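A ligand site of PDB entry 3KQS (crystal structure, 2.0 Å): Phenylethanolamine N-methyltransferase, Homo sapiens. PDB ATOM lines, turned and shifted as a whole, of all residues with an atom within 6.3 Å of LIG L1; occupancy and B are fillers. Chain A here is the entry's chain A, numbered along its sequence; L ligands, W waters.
The side-chain carboxylate (OD2) of Asp 77 lies within hydrogen-bond range of the side-chain hydroxyl (OG) of Ser 80 (2.6 Å). The backbone NH (N) of Ile 157 lies within hydrogen-bond range of the backbone carbonyl oxygen (O) of Asp 101, 3.3 Å away. The side-chain amide oxygen (OE1) of Gln 86 sits at hydrogen-bond distance from the side-chain hydroxyl (OG1) of Thr 83 (2.7 Å). O of Val 187 lies within hydrogen-bond range of NE2 of His 160, at 2.8 Å. N of His 160 is in hydrogen-bond range of OD1 of Asp 158, at 2.9 Å. The side-chain carboxylate of Asp 101 lies within hydrogen-bond range of the backbone NH of Leu 103. OH of Tyr 27 is in hydrogen-bond range of O of Ala 186, 2.7 Å away. The backbone carbonyl oxygen of Ser 80 sits at hydrogen-bond distance from the side-chain hydroxyl of Thr 83 (3.3 Å).
N1 of LIG L1 sits at hydrogen-bond distance from O of Ala 181, at 2.8 Å. An oxygen (O1) of LIG L1 sits close to the side-chain hydroxyl (OG1) of Thr 83 (3.5 Å). O4 of LIG L1 is in hydrogen-bond range of OD1 of Asn 106, 3.1 Å away. A nitrogen (N3) of LG2 L2 is in hydrogen-bond range of the side-chain hydroxyl (OH) of Tyr 35. OH of Tyr 85 sits at hydrogen-bond distance from O1 of LIG L1 (2.8 Å). The side-chain sulfur (SG) of Cys 183 sits at hydrogen-bond distance from a nitrogen (N6) of LIG L1 (3.4 Å). O of Gly 79 lies within hydrogen-bond range of N1 of LIG L1 (2.8 Å). The side-chain carboxylate (OD1) of Asp 158 is in hydrogen-bond range of a nitrogen (N4) of LIG L1 (2.8 Å). The backbone NH (N) of Val 159 sits at hydrogen-bond distance from a nitrogen (N5) of LIG L1 (2.8 Å). OH of Tyr 40 sits at hydrogen-bond distance from N1 of LG2 L2 (2.9 Å). O2 of LIG L1 is in hydrogen-bond range of OH of Tyr 35. The side-chain hydroxyl (OH) of Tyr 40 is in hydrogen-bond range of an oxygen (O2) of LIG L1. N1 of LIG L1 lies close to O of Ser 80 (3.2 Å). OD1 of Asp 101 is in hydrogen-bond range of O4 of LIG L1 (2.8 Å).
S1 of LIG L1 lies close to O of Phe 182 (3.7 Å). Residues that only touch LIG L1: Gly 81, His 160, Phe 102, Val 187, Leu 103, Tyr 27, Ile 157, Gln 86 and Tyr 222. Hydrophobic or aromatic side chains within 4 Å of LIG L1: Tyr 27, Tyr 35, Tyr 40, Tyr 85, Phe 102, Leu 103, Ile 157, Val 159, His 160, Ala 181, Phe 182 and Val 187. Within 4 Å of LIG L1: Tyr 27, Tyr 35, Tyr 40, Gly 79, Ser 80, Gly 81, Thr 83, Tyr 85, Gln 86, Asp 101, Phe 102, Leu 103, Asn 106, Ile 157, Asp 158, Val 159, His 160, Ala 181, Phe 182, Cys 183, Val 187 and Tyr 222.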
ATOM      1  N   ALA A  24     -13.325 -20.031  13.137  1.00  0.00           N
ATOM      2  CA  ALA A  24     -13.834 -21.397  13.218  1.00  0.00           C
ATOM      3  C   ALA A  24     -13.476 -22.039  14.560  1.00  0.00           C
ATOM      4  O   ALA A  24     -14.248 -22.831  15.098  1.00  0.00           O
ATOM      5  CB  ALA A  24     -13.300 -22.233  12.067  1.00  0.00           C
ATOM      6  N   TYR A  27     -15.802 -23.173  17.188  1.00  0.00           N
ATOM      7  CA  TYR A  27     -16.542 -24.434  17.161  1.00  0.00           C
ATOM      8  C   TYR A  27     -15.911 -25.544  18.005  1.00  0.00           C
ATOM      9  O   TYR A  27     -16.583 -26.513  18.363  1.00  0.00           O
ATOM     10  CB  TYR A  27     -16.799 -24.907  15.729  1.00  0.00           C
ATOM     11  CG  TYR A  27     -18.096 -24.336  15.197  1.00  0.00           C
ATOM     12  CD1 TYR A  27     -18.094 -23.275  14.302  1.00  0.00           C
ATOM     13  CD2 TYR A  27     -19.316 -24.834  15.631  1.00  0.00           C
ATOM     14  CE1 TYR A  27     -19.277 -22.747  13.832  1.00  0.00           C
ATOM     15  CE2 TYR A  27     -20.500 -24.299  15.173  1.00  0.00           C
ATOM     16  CZ  TYR A  27     -20.471 -23.258  14.275  1.00  0.00           C
ATOM     17  OH  TYR A  27     -21.655 -22.723  13.816  1.00  0.00           O
ATOM     18  N   PHE A  30     -17.976 -25.965  20.988  1.00  0.00           N
ATOM     19  CA  PHE A  30     -19.364 -26.386  20.747  1.00  0.00           C
ATOM     20  C   PHE A  30     -19.724 -27.627  21.553  1.00  0.00           C
ATOM     21  O   PHE A  30     -19.106 -28.680  21.391  1.00  0.00           O
ATOM     22  CB  PHE A  30     -19.543 -26.646  19.247  1.00  0.00           C
ATOM     23  CG  PHE A  30     -20.949 -26.960  18.821  1.00  0.00           C
ATOM     24  CD1 PHE A  30     -21.737 -25.985  18.229  1.00  0.00           C
ATOM     25  CD2 PHE A  30     -21.466 -28.235  18.971  1.00  0.00           C
ATOM     26  CE1 PHE A  30     -23.025 -26.265  17.824  1.00  0.00           C
ATOM     27  CE2 PHE A  30     -22.762 -28.529  18.558  1.00  0.00           C
ATOM     28  CZ  PHE A  30     -23.545 -27.546  17.986  1.00  0.00           C
ATOM     29  N   TYR A  35     -26.419 -27.474  22.878  1.00  0.00           N
ATOM     30  CA  TYR A  35     -27.058 -27.103  21.614  1.00  0.00           C
ATOM     31  C   TYR A  35     -28.442 -27.762  21.464  1.00  0.00           C
ATOM     32  O   TYR A  35     -29.414 -27.103  21.087  1.00  0.00           O
ATOM     33  CB  TYR A  35     -26.174 -27.479  20.433  1.00  0.00           C
ATOM     34  CG  TYR A  35     -26.802 -27.200  19.076  1.00  0.00           C
ATOM     35  CD1 TYR A  35     -26.809 -25.910  18.556  1.00  0.00           C
ATOM     36  CD2 TYR A  35     -27.385 -28.223  18.332  1.00  0.00           C
ATOM     37  CE1 TYR A  35     -27.380 -25.647  17.327  1.00  0.00           C
ATOM     38  CE2 TYR A  35     -27.956 -27.960  17.102  1.00  0.00           C
ATOM     39  CZ  TYR A  35     -27.961 -26.677  16.603  1.00  0.00           C
ATOM     40  OH  TYR A  35     -28.524 -26.401  15.383  1.00  0.00           O
ATOM     41  N   ASN A  39     -32.326 -25.784  21.516  1.00  0.00           N
ATOM     42  CA  ASN A  39     -33.071 -25.658  20.263  1.00  0.00           C
ATOM     43  C   ASN A  39     -34.143 -26.717  20.008  1.00  0.00           C
ATOM     44  O   ASN A  39     -35.051 -26.488  19.200  1.00  0.00           O
ATOM     45  CB  ASN A  39     -32.104 -25.610  19.075  1.00  0.00           C
ATOM     46  CG  ASN A  39     -31.190 -24.406  19.131  1.00  0.00           C
ATOM     47  OD1 ASN A  39     -31.612 -23.290  18.869  1.00  0.00           O
ATOM     48  ND2 ASN A  39     -29.938 -24.632  19.512  1.00  0.00           N
ATOM     49  N   TYR A  40     -34.035 -27.851  20.681  1.00  0.00           N
ATOM     50  CA  TYR A  40     -34.884 -29.009  20.380  1.00  0.00           C
ATOM     51  C   TYR A  40     -35.522 -29.624  21.609  1.00  0.00           C
ATOM     52  O   TYR A  40     -36.093 -30.720  21.554  1.00  0.00           O
ATOM     53  CB  TYR A  40     -34.095 -30.043  19.555  1.00  0.00           C
ATOM     54  CG  TYR A  40     -33.530 -29.398  18.298  1.00  0.00           C
ATOM     55  CD1 TYR A  40     -32.206 -29.001  18.219  1.00  0.00           C
ATOM     56  CD2 TYR A  40     -34.357 -29.128  17.214  1.00  0.00           C
ATOM     57  CE1 TYR A  40     -31.699 -28.392  17.069  1.00  0.00           C
ATOM     58  CE2 TYR A  40     -33.867 -28.516  16.061  1.00  0.00           C
ATOM     59  CZ  TYR A  40     -32.539 -28.147  16.000  1.00  0.00           C
ATOM     60  OH  TYR A  40     -32.056 -27.534  14.863  1.00  0.00           O
ATOM     61  N   LYS A  57     -41.188 -26.322  10.514  1.00  0.00           N
ATOM     62  CA  LYS A  57     -40.079 -26.950   9.794  1.00  0.00           C
ATOM     63  C   LYS A  57     -40.438 -28.327   9.231  1.00  0.00           C
ATOM     64  O   LYS A  57     -40.138 -28.629   8.077  1.00  0.00           O
ATOM     65  CB  LYS A  57     -38.839 -27.066  10.699  1.00  0.00           C
ATOM     66  CG  LYS A  57     -38.095 -25.743  10.921  1.00  0.00           C
ATOM     67  CD  LYS A  57     -36.779 -25.973  11.665  1.00  0.00           C
ATOM     68  CE  LYS A  57     -37.050 -26.509  13.071  1.00  0.00           C
ATOM     69  NZ  LYS A  57     -35.793 -26.735  13.811  1.00  0.00           N
ATOM     70  N   ASP A  77     -26.864 -35.041   3.716  1.00  0.00           N
ATOM     71  CA  ASP A  77     -27.233 -33.992   4.675  1.00  0.00           C
ATOM     72  C   ASP A  77     -25.969 -33.237   5.065  1.00  0.00           C
ATOM     73  O   ASP A  77     -25.009 -33.825   5.556  1.00  0.00           O
ATOM     74  CB  ASP A  77     -27.882 -34.619   5.920  1.00  0.00           C
ATOM     75  CG  ASP A  77     -28.372 -33.572   6.930  1.00  0.00           C
ATOM     76  OD1 ASP A  77     -28.752 -32.469   6.509  1.00  0.00           O
ATOM     77  OD2 ASP A  77     -28.369 -33.868   8.136  1.00  0.00           O
ATOM     78  N   ILE A  78     -25.977 -31.919   4.819  1.00  0.00           N
ATOM     79  CA  ILE A  78     -24.804 -31.063   5.027  1.00  0.00           C
ATOM     80  C   ILE A  78     -24.805 -30.363   6.375  1.00  0.00           C
ATOM     81  O   ILE A  78     -25.720 -29.591   6.680  1.00  0.00           O
ATOM     82  CB  ILE A  78     -24.750 -29.952   3.951  1.00  0.00           C
ATOM     83  CG1 ILE A  78     -24.844 -30.546   2.537  1.00  0.00           C
ATOM     84  CG2 ILE A  78     -23.492 -29.107   4.126  1.00  0.00           C
ATOM     85  CD1 ILE A  78     -23.637 -31.375   2.144  1.00  0.00           C
ATOM     86  N   GLY A  79     -23.776 -30.611   7.187  1.00  0.00           N
ATOM     87  CA  GLY A  79     -23.692 -30.010   8.505  1.00  0.00           C
ATOM     88  C   GLY A  79     -24.817 -30.479   9.424  1.00  0.00           C
ATOM     89  O   GLY A  79     -25.558 -29.672   9.991  1.00  0.00           O
ATOM     90  N   SER A  80     -24.932 -31.803   9.564  1.00  0.00           N
ATOM     91  CA  SER A  80     -25.999 -32.418  10.349  1.00  0.00           C
ATOM     92  C   SER A  80     -25.962 -32.035  11.821  1.00  0.00           C
ATOM     93  O   SER A  80     -26.993 -32.017  12.483  1.00  0.00           O
ATOM     94  CB  SER A  80     -25.892 -33.940  10.255  1.00  0.00           C
ATOM     95  OG  SER A  80     -25.900 -34.391   8.910  1.00  0.00           O
ATOM     96  N   GLY A  81     -24.776 -31.745  12.336  1.00  0.00           N
ATOM     97  CA  GLY A  81     -24.628 -31.588  13.776  1.00  0.00           C
ATOM     98  C   GLY A  81     -25.124 -32.847  14.459  1.00  0.00           C
ATOM     99  O   GLY A  81     -24.984 -33.945  13.931  1.00  0.00           O
ATOM    100  N   PRO A  82     -25.739 -32.687  15.651  1.00  0.00           N
ATOM    101  CA  PRO A  82     -26.274 -33.827  16.409  1.00  0.00           C
ATOM    102  C   PRO A  82     -27.775 -34.073  16.174  1.00  0.00           C
ATOM    103  O   PRO A  82     -28.403 -34.677  17.038  1.00  0.00           O
ATOM    104  CB  PRO A  82     -26.055 -33.389  17.847  1.00  0.00           C
ATOM    105  CG  PRO A  82     -26.230 -31.878  17.806  1.00  0.00           C
ATOM    106  CD  PRO A  82     -25.840 -31.424  16.410  1.00  0.00           C
ATOM    107  N   THR A  83     -28.327 -33.623  15.053  1.00  0.00           N
ATOM    108  CA  THR A  83     -29.774 -33.698  14.861  1.00  0.00           C
ATOM    109  C   THR A  83     -30.188 -34.587  13.690  1.00  0.00           C
ATOM    110  O   THR A  83     -29.424 -34.765  12.735  1.00  0.00           O
ATOM    111  CB  THR A  83     -30.407 -32.290  14.665  1.00  0.00           C
ATOM    112  OG1 THR A  83     -30.123 -31.804  13.349  1.00  0.00           O
ATOM    113  CG2 THR A  83     -29.868 -31.315  15.699  1.00  0.00           C
ATOM    114  N   TYR A  85     -33.938 -34.626  12.856  1.00  0.00           N
ATOM    115  CA  TYR A  85     -35.297 -34.196  12.481  1.00  0.00           C
ATOM    116  C   TYR A  85     -35.362 -33.808  10.999  1.00  0.00           C
ATOM    117  O   TYR A  85     -36.405 -33.972  10.363  1.00  0.00           O
ATOM    118  CB  TYR A  85     -35.777 -33.011  13.328  1.00  0.00           C
ATOM    119  CG  TYR A  85     -35.098 -31.711  12.938  1.00  0.00           C
ATOM    120  CD1 TYR A  85     -35.658 -30.864  12.001  1.00  0.00           C
ATOM    121  CD2 TYR A  85     -33.857 -31.374  13.474  1.00  0.00           C
ATOM    122  CE1 TYR A  85     -35.025 -29.699  11.612  1.00  0.00           C
ATOM    123  CE2 TYR A  85     -33.211 -30.212  13.078  1.00  0.00           C
ATOM    124  CZ  TYR A  85     -33.799 -29.374  12.155  1.00  0.00           C
ATOM    125  OH  TYR A  85     -33.165 -28.216  11.754  1.00  0.00           O
ATOM    126  N   GLN A  86     -34.262 -33.294  10.470  1.00  0.00           N
ATOM    127  CA  GLN A  86     -34.238 -32.785   9.088  1.00  0.00           C
ATOM    128  C   GLN A  86     -34.351 -33.872   8.026  1.00  0.00           C
ATOM    129  O   GLN A  86     -34.533 -33.567   6.846  1.00  0.00           O
ATOM    130  CB  GLN A  86     -32.993 -31.926   8.852  1.00  0.00           C
ATOM    131  CG  GLN A  86     -31.663 -32.683   8.899  1.00  0.00           C
ATOM    132  CD  GLN A  86     -31.020 -32.647  10.274  1.00  0.00           C
ATOM    133  OE1 GLN A  86     -31.696 -32.500  11.283  1.00  0.00           O
ATOM    134  NE2 GLN A  86     -29.697 -32.759  10.300  1.00  0.00           N
ATOM    135  N   ASP A 101     -20.745 -33.933   9.500  1.00  0.00           N
ATOM    136  CA  ASP A 101     -20.464 -32.750  10.302  1.00  0.00           C
ATOM    137  C   ASP A 101     -18.989 -32.466  10.429  1.00  0.00           C
ATOM    138  O   ASP A 101     -18.147 -33.348  10.278  1.00  0.00           O
ATOM    139  CB  ASP A 101     -21.100 -32.819  11.689  1.00  0.00           C
ATOM    140  CG  ASP A 101     -21.247 -31.435  12.313  1.00  0.00           C
ATOM    141  OD1 ASP A 101     -22.068 -30.653  11.800  1.00  0.00           O
ATOM    142  OD2 ASP A 101     -20.538 -31.133  13.303  1.00  0.00           O
ATOM    143  N   PHE A 102     -18.686 -31.214  10.728  1.00  0.00           N
ATOM    144  CA  PHE A 102     -17.326 -30.745  10.897  1.00  0.00           C
ATOM    145  C   PHE A 102     -16.742 -31.261  12.211  1.00  0.00           C
ATOM    146  O   PHE A 102     -15.539 -31.506  12.311  1.00  0.00           O
ATOM    147  CB  PHE A 102     -17.313 -29.216  10.861  1.00  0.00           C
ATOM    148  CG  PHE A 102     -15.964 -28.599  11.071  1.00  0.00           C
ATOM    149  CD1 PHE A 102     -15.038 -28.560  10.038  1.00  0.00           C
ATOM    150  CD2 PHE A 102     -15.631 -28.039  12.290  1.00  0.00           C
ATOM    151  CE1 PHE A 102     -13.797 -27.986  10.233  1.00  0.00           C
ATOM    152  CE2 PHE A 102     -14.380 -27.473  12.490  1.00  0.00           C
ATOM    153  CZ  PHE A 102     -13.467 -27.440  11.453  1.00  0.00           C
ATOM    154  N   LEU A 103     -17.597 -31.431  13.218  1.00  0.00           N
ATOM    155  CA  LEU A 103     -17.122 -31.802  14.556  1.00  0.00           C
ATOM    156  C   LEU A 103     -17.286 -33.285  14.855  1.00  0.00           C
ATOM    157  O   LEU A 103     -18.343 -33.884  14.619  1.00  0.00           O
ATOM    158  CB  LEU A 103     -17.840 -30.980  15.632  1.00  0.00           C
ATOM    159  CG  LEU A 103     -17.495 -29.490  15.680  1.00  0.00           C
ATOM    160  CD1 LEU A 103     -18.344 -28.778  16.725  1.00  0.00           C
ATOM    161  CD2 LEU A 103     -16.005 -29.291  15.962  1.00  0.00           C
ATOM    162  N   ASN A 106     -20.070 -34.138  17.338  1.00  0.00           N
ATOM    163  CA  ASN A 106     -21.402 -34.212  16.736  1.00  0.00           C
ATOM    164  C   ASN A 106     -21.620 -35.542  16.036  1.00  0.00           C
ATOM    165  O   ASN A 106     -22.695 -36.151  16.148  1.00  0.00           O
ATOM    166  CB  ASN A 106     -21.630 -33.038  15.779  1.00  0.00           C
ATOM    167  CG  ASN A 106     -22.050 -31.767  16.489  1.00  0.00           C
ATOM    168  OD1 ASN A 106     -21.769 -30.653  16.030  1.00  0.00           O
ATOM    169  ND2 ASN A 106     -22.704 -31.919  17.619  1.00  0.00           N
ATOM    170  N   ILE A 157     -16.865 -33.131   7.279  1.00  0.00           N
ATOM    171  CA  ILE A 157     -17.132 -32.213   6.173  1.00  0.00           C
ATOM    172  C   ILE A 157     -16.672 -30.798   6.528  1.00  0.00           C
ATOM    173  O   ILE A 157     -16.726 -30.396   7.687  1.00  0.00           O
ATOM    174  CB  ILE A 157     -18.620 -32.205   5.795  1.00  0.00           C
ATOM    175  CG1 ILE A 157     -18.855 -31.377   4.529  1.00  0.00           C
ATOM    176  CG2 ILE A 157     -19.464 -31.679   6.956  1.00  0.00           C
ATOM    177  CD1 ILE A 157     -20.250 -31.502   3.967  1.00  0.00           C
ATOM    178  N   ASP A 158     -16.214 -30.052   5.517  1.00  0.00           N
ATOM    179  CA  ASP A 158     -15.873 -28.645   5.684  1.00  0.00           C
ATOM    180  C   ASP A 158     -16.339 -27.869   4.466  1.00  0.00           C
ATOM    181  O   ASP A 158     -15.699 -27.901   3.419  1.00  0.00           O
ATOM    182  CB  ASP A 158     -14.357 -28.477   5.859  1.00  0.00           C
ATOM    183  CG  ASP A 158     -13.958 -27.022   6.114  1.00  0.00           C
ATOM    184  OD1 ASP A 158     -14.831 -26.138   6.055  1.00  0.00           O
ATOM    185  OD2 ASP A 158     -12.756 -26.771   6.370  1.00  0.00           O
ATOM    186  N   VAL A 159     -17.466 -27.165   4.604  1.00  0.00           N
ATOM    187  CA  VAL A 159     -18.065 -26.467   3.460  1.00  0.00           C
ATOM    188  C   VAL A 159     -17.194 -25.319   2.957  1.00  0.00           C
ATOM    189  O   VAL A 159     -17.484 -24.728   1.914  1.00  0.00           O
ATOM    190  CB  VAL A 159     -19.473 -25.931   3.785  1.00  0.00           C
ATOM    191  CG1 VAL A 159     -20.419 -27.080   4.180  1.00  0.00           C
ATOM    192  CG2 VAL A 159     -19.401 -24.885   4.865  1.00  0.00           C
ATOM    193  N   HIS A 160     -16.143 -24.995   3.692  1.00  0.00           N
ATOM    194  CA  HIS A 160     -15.214 -23.951   3.264  1.00  0.00           C
ATOM    195  C   HIS A 160     -14.211 -24.478   2.245  1.00  0.00           C
ATOM    196  O   HIS A 160     -13.526 -23.700   1.582  1.00  0.00           O
ATOM    197  CB  HIS A 160     -14.493 -23.336   4.466  1.00  0.00           C
ATOM    198  CG  HIS A 160     -15.396 -22.587   5.395  1.00  0.00           C
ATOM    199  ND1 HIS A 160     -16.293 -21.642   4.947  1.00  0.00           N
ATOM    200  CD2 HIS A 160     -15.539 -22.639   6.731  1.00  0.00           C
ATOM    201  CE1 HIS A 160     -16.953 -21.145   5.977  1.00  0.00           C
ATOM    202  NE2 HIS A 160     -16.509 -21.731   7.075  1.00  0.00           N
ATOM    203  N   SER A 180     -29.794 -29.381   4.125  1.00  0.00           N
ATOM    204  CA  SER A 180     -28.884 -28.682   5.034  1.00  0.00           C
ATOM    205  C   SER A 180     -29.666 -27.708   5.896  1.00  0.00           C
ATOM    206  O   SER A 180     -30.410 -26.877   5.370  1.00  0.00           O
ATOM    207  CB  SER A 180     -27.795 -27.957   4.246  1.00  0.00           C
ATOM    208  OG  SER A 180     -26.847 -27.354   5.115  1.00  0.00           O
ATOM    209  N   ALA A 181     -29.496 -27.790   7.202  1.00  0.00           N
ATOM    210  CA  ALA A 181     -30.266 -26.932   8.105  1.00  0.00           C
ATOM    211  C   ALA A 181     -29.366 -26.215   9.111  1.00  0.00           C
ATOM    212  O   ALA A 181     -28.628 -26.851   9.849  1.00  0.00           O
ATOM    213  CB  ALA A 181     -31.357 -27.732   8.831  1.00  0.00           C
ATOM    214  N   PHE A 182     -29.458 -24.880   9.113  1.00  0.00           N
ATOM    215  CA  PHE A 182     -28.774 -24.038  10.106  1.00  0.00           C
ATOM    216  C   PHE A 182     -27.245 -24.145  10.070  1.00  0.00           C
ATOM    217  O   PHE A 182     -26.580 -23.898  11.079  1.00  0.00           O
ATOM    218  CB  PHE A 182     -29.295 -24.341  11.515  1.00  0.00           C
ATOM    219  CG  PHE A 182     -30.768 -24.068  11.706  1.00  0.00           C
ATOM    220  CD1 PHE A 182     -31.655 -25.119  11.897  1.00  0.00           C
ATOM    221  CD2 PHE A 182     -31.252 -22.766  11.694  1.00  0.00           C
ATOM    222  CE1 PHE A 182     -33.008 -24.865  12.091  1.00  0.00           C
ATOM    223  CE2 PHE A 182     -32.609 -22.511  11.880  1.00  0.00           C
ATOM    224  CZ  PHE A 182     -33.487 -23.571  12.077  1.00  0.00           C
ATOM    225  N   CYS A 183     -26.686 -24.494   8.914  1.00  0.00           N
ATOM    226  CA  CYS A 183     -25.232 -24.646   8.789  1.00  0.00           C
ATOM    227  C   CYS A 183     -24.537 -23.458   8.109  1.00  0.00           C
ATOM    228  O   CYS A 183     -23.694 -22.782   8.723  1.00  0.00           O
ATOM    229  CB  CYS A 183     -24.871 -25.947   8.072  1.00  0.00           C
ATOM    230  SG  CYS A 183     -23.095 -26.207   7.782  1.00  0.00           S
ATOM    231  N   LEU A 184     -24.871 -23.195   6.847  1.00  0.00           N
ATOM    232  CA  LEU A 184     -24.094 -22.222   6.062  1.00  0.00           C
ATOM    233  C   LEU A 184     -23.975 -20.850   6.727  1.00  0.00           C
ATOM    234  O   LEU A 184     -22.879 -20.305   6.847  1.00  0.00           O
ATOM    235  CB  LEU A 184     -24.647 -22.083   4.643  1.00  0.00           C
ATOM    236  CG  LEU A 184     -24.759 -23.374   3.835  1.00  0.00           C
ATOM    237  CD1 LEU A 184     -25.185 -23.053   2.410  1.00  0.00           C
ATOM    238  CD2 LEU A 184     -23.442 -24.151   3.853  1.00  0.00           C
ATOM    239  N   ALA A 186     -24.283 -20.203   9.745  1.00  0.00           N
ATOM    240  CA  ALA A 186     -23.677 -20.384  11.065  1.00  0.00           C
ATOM    241  C   ALA A 186     -22.169 -20.595  11.020  1.00  0.00           C
ATOM    242  O   ALA A 186     -21.521 -20.663  12.067  1.00  0.00           O
ATOM    243  CB  ALA A 186     -24.368 -21.543  11.801  1.00  0.00           C
ATOM    244  N   VAL A 187     -21.610 -20.722   9.814  1.00  0.00           N
ATOM    245  CA  VAL A 187     -20.178 -20.963   9.670  1.00  0.00           C
ATOM    246  C   VAL A 187     -19.485 -19.940   8.752  1.00  0.00           C
ATOM    247  O   VAL A 187     -18.283 -20.056   8.479  1.00  0.00           O
ATOM    248  CB  VAL A 187     -19.888 -22.403   9.183  1.00  0.00           C
ATOM    249  CG1 VAL A 187     -20.638 -23.415  10.052  1.00  0.00           C
ATOM    250  CG2 VAL A 187     -20.286 -22.565   7.737  1.00  0.00           C
ATOM    251  N   TYR A 222     -25.277 -17.325  18.350  1.00  0.00           N
ATOM    252  CA  TYR A 222     -25.978 -18.306  19.175  1.00  0.00           C
ATOM    253  C   TYR A 222     -25.000 -18.987  20.134  1.00  0.00           C
ATOM    254  O   TYR A 222     -23.787 -18.952  19.924  1.00  0.00           O
ATOM    255  CB  TYR A 222     -26.750 -19.335  18.325  1.00  0.00           C
ATOM    256  CG  TYR A 222     -25.903 -20.364  17.605  1.00  0.00           C
ATOM    257  CD1 TYR A 222     -25.835 -21.674  18.080  1.00  0.00           C
ATOM    258  CD2 TYR A 222     -25.212 -20.047  16.447  1.00  0.00           C
ATOM    259  CE1 TYR A 222     -25.077 -22.632  17.424  1.00  0.00           C
ATOM    260  CE2 TYR A 222     -24.454 -21.012  15.779  1.00  0.00           C
ATOM    261  CZ  TYR A 222     -24.383 -22.294  16.278  1.00  0.00           C
ATOM    262  OH  TYR A 222     -23.650 -23.253  15.623  1.00  0.00           O
HETATM  263  N1  LIG L   1     -28.092 -29.356  11.053  1.00  0.00           N
HETATM  264  C1  LIG L   1     -28.205 -29.245  12.512  1.00  0.00           C
HETATM  265  C2  LIG L   1     -26.969 -28.522  13.106  1.00  0.00           C
HETATM  266  C3  LIG L   1     -26.979 -27.017  12.809  1.00  0.00           C
HETATM  267  S1  LIG L   1     -25.687 -26.187  13.812  1.00  0.00           S
HETATM  268  C4  LIG L   1     -29.524 -28.523  12.863  1.00  0.00           C
HETATM  269  O1  LIG L   1     -30.436 -28.567  12.102  1.00  0.00           O
HETATM  270  O2  LIG L   1     -29.774 -28.278  14.212  1.00  0.00           O
HETATM  271  C5  LIG L   1     -24.308 -25.710  12.739  1.00  0.00           C
HETATM  272  C6  LIG L   1     -23.432 -26.937  12.429  1.00  0.00           C
HETATM  273  O3  LIG L   1     -22.395 -26.573  11.467  1.00  0.00           O
HETATM  274  C7  LIG L   1     -22.712 -27.513  13.655  1.00  0.00           C
HETATM  275  O4  LIG L   1     -23.030 -28.882  13.773  1.00  0.00           O
HETATM  276  C8  LIG L   1     -21.247 -27.325  13.316  1.00  0.00           C
HETATM  277  O5  LIG L   1     -20.442 -28.335  13.864  1.00  0.00           O
HETATM  278  C9  LIG L   1     -21.270 -27.417  11.794  1.00  0.00           C
HETATM  279  N2  LIG L   1     -20.086 -26.791  11.254  1.00  0.00           N
HETATM  280  C10 LIG L   1     -19.138 -25.854  11.937  1.00  0.00           C
HETATM  281  N3  LIG L   1     -18.100 -25.490  10.976  1.00  0.00           N
HETATM  282  C11 LIG L   1     -18.400 -26.181   9.706  1.00  0.00           C
HETATM  283  C12 LIG L   1     -17.714 -26.201   8.375  1.00  0.00           C
HETATM  284  N4  LIG L   1     -16.515 -25.411   8.157  1.00  0.00           N
HETATM  285  N5  LIG L   1     -18.275 -26.999   7.288  1.00  0.00           N
HETATM  286  C13 LIG L   1     -19.522 -27.808   7.484  1.00  0.00           C
HETATM  287  N6  LIG L   1     -20.208 -27.796   8.803  1.00  0.00           N
HETATM  288  C14 LIG L   1     -19.640 -26.985   9.898  1.00  0.00           C
HETATM  289  N1  LG2 L   2     -32.029 -24.699  15.417  1.00  0.00           N
HETATM  290  C1  LG2 L   2     -33.310 -23.995  15.679  1.00  0.00           C
HETATM  291  C2  LG2 L   2     -34.644 -24.488  15.902  1.00  0.00           C
HETATM  292  C3  LG2 L   2     -35.732 -23.566  16.127  1.00  0.00           C
HETATM  293  C4  LG2 L   2     -35.474 -22.138  16.148  1.00  0.00           C
HETATM  294  C5  LG2 L   2     -34.140 -21.645  15.925  1.00  0.00           C
HETATM  295  C6  LG2 L   2     -33.061 -22.558  15.694  1.00  0.00           C
HETATM  296  N2  LG2 L   2     -31.574 -22.343  15.447  1.00  0.00           N
HETATM  297  C7  LG2 L   2     -30.950 -23.665  15.271  1.00  0.00           C
HETATM  298  N3  LG2 L   2     -29.539 -23.912  15.014  1.00  0.00           N
HETATM  299  O   HOH W   1     -15.771 -24.189  11.276  1.00  0.00           O
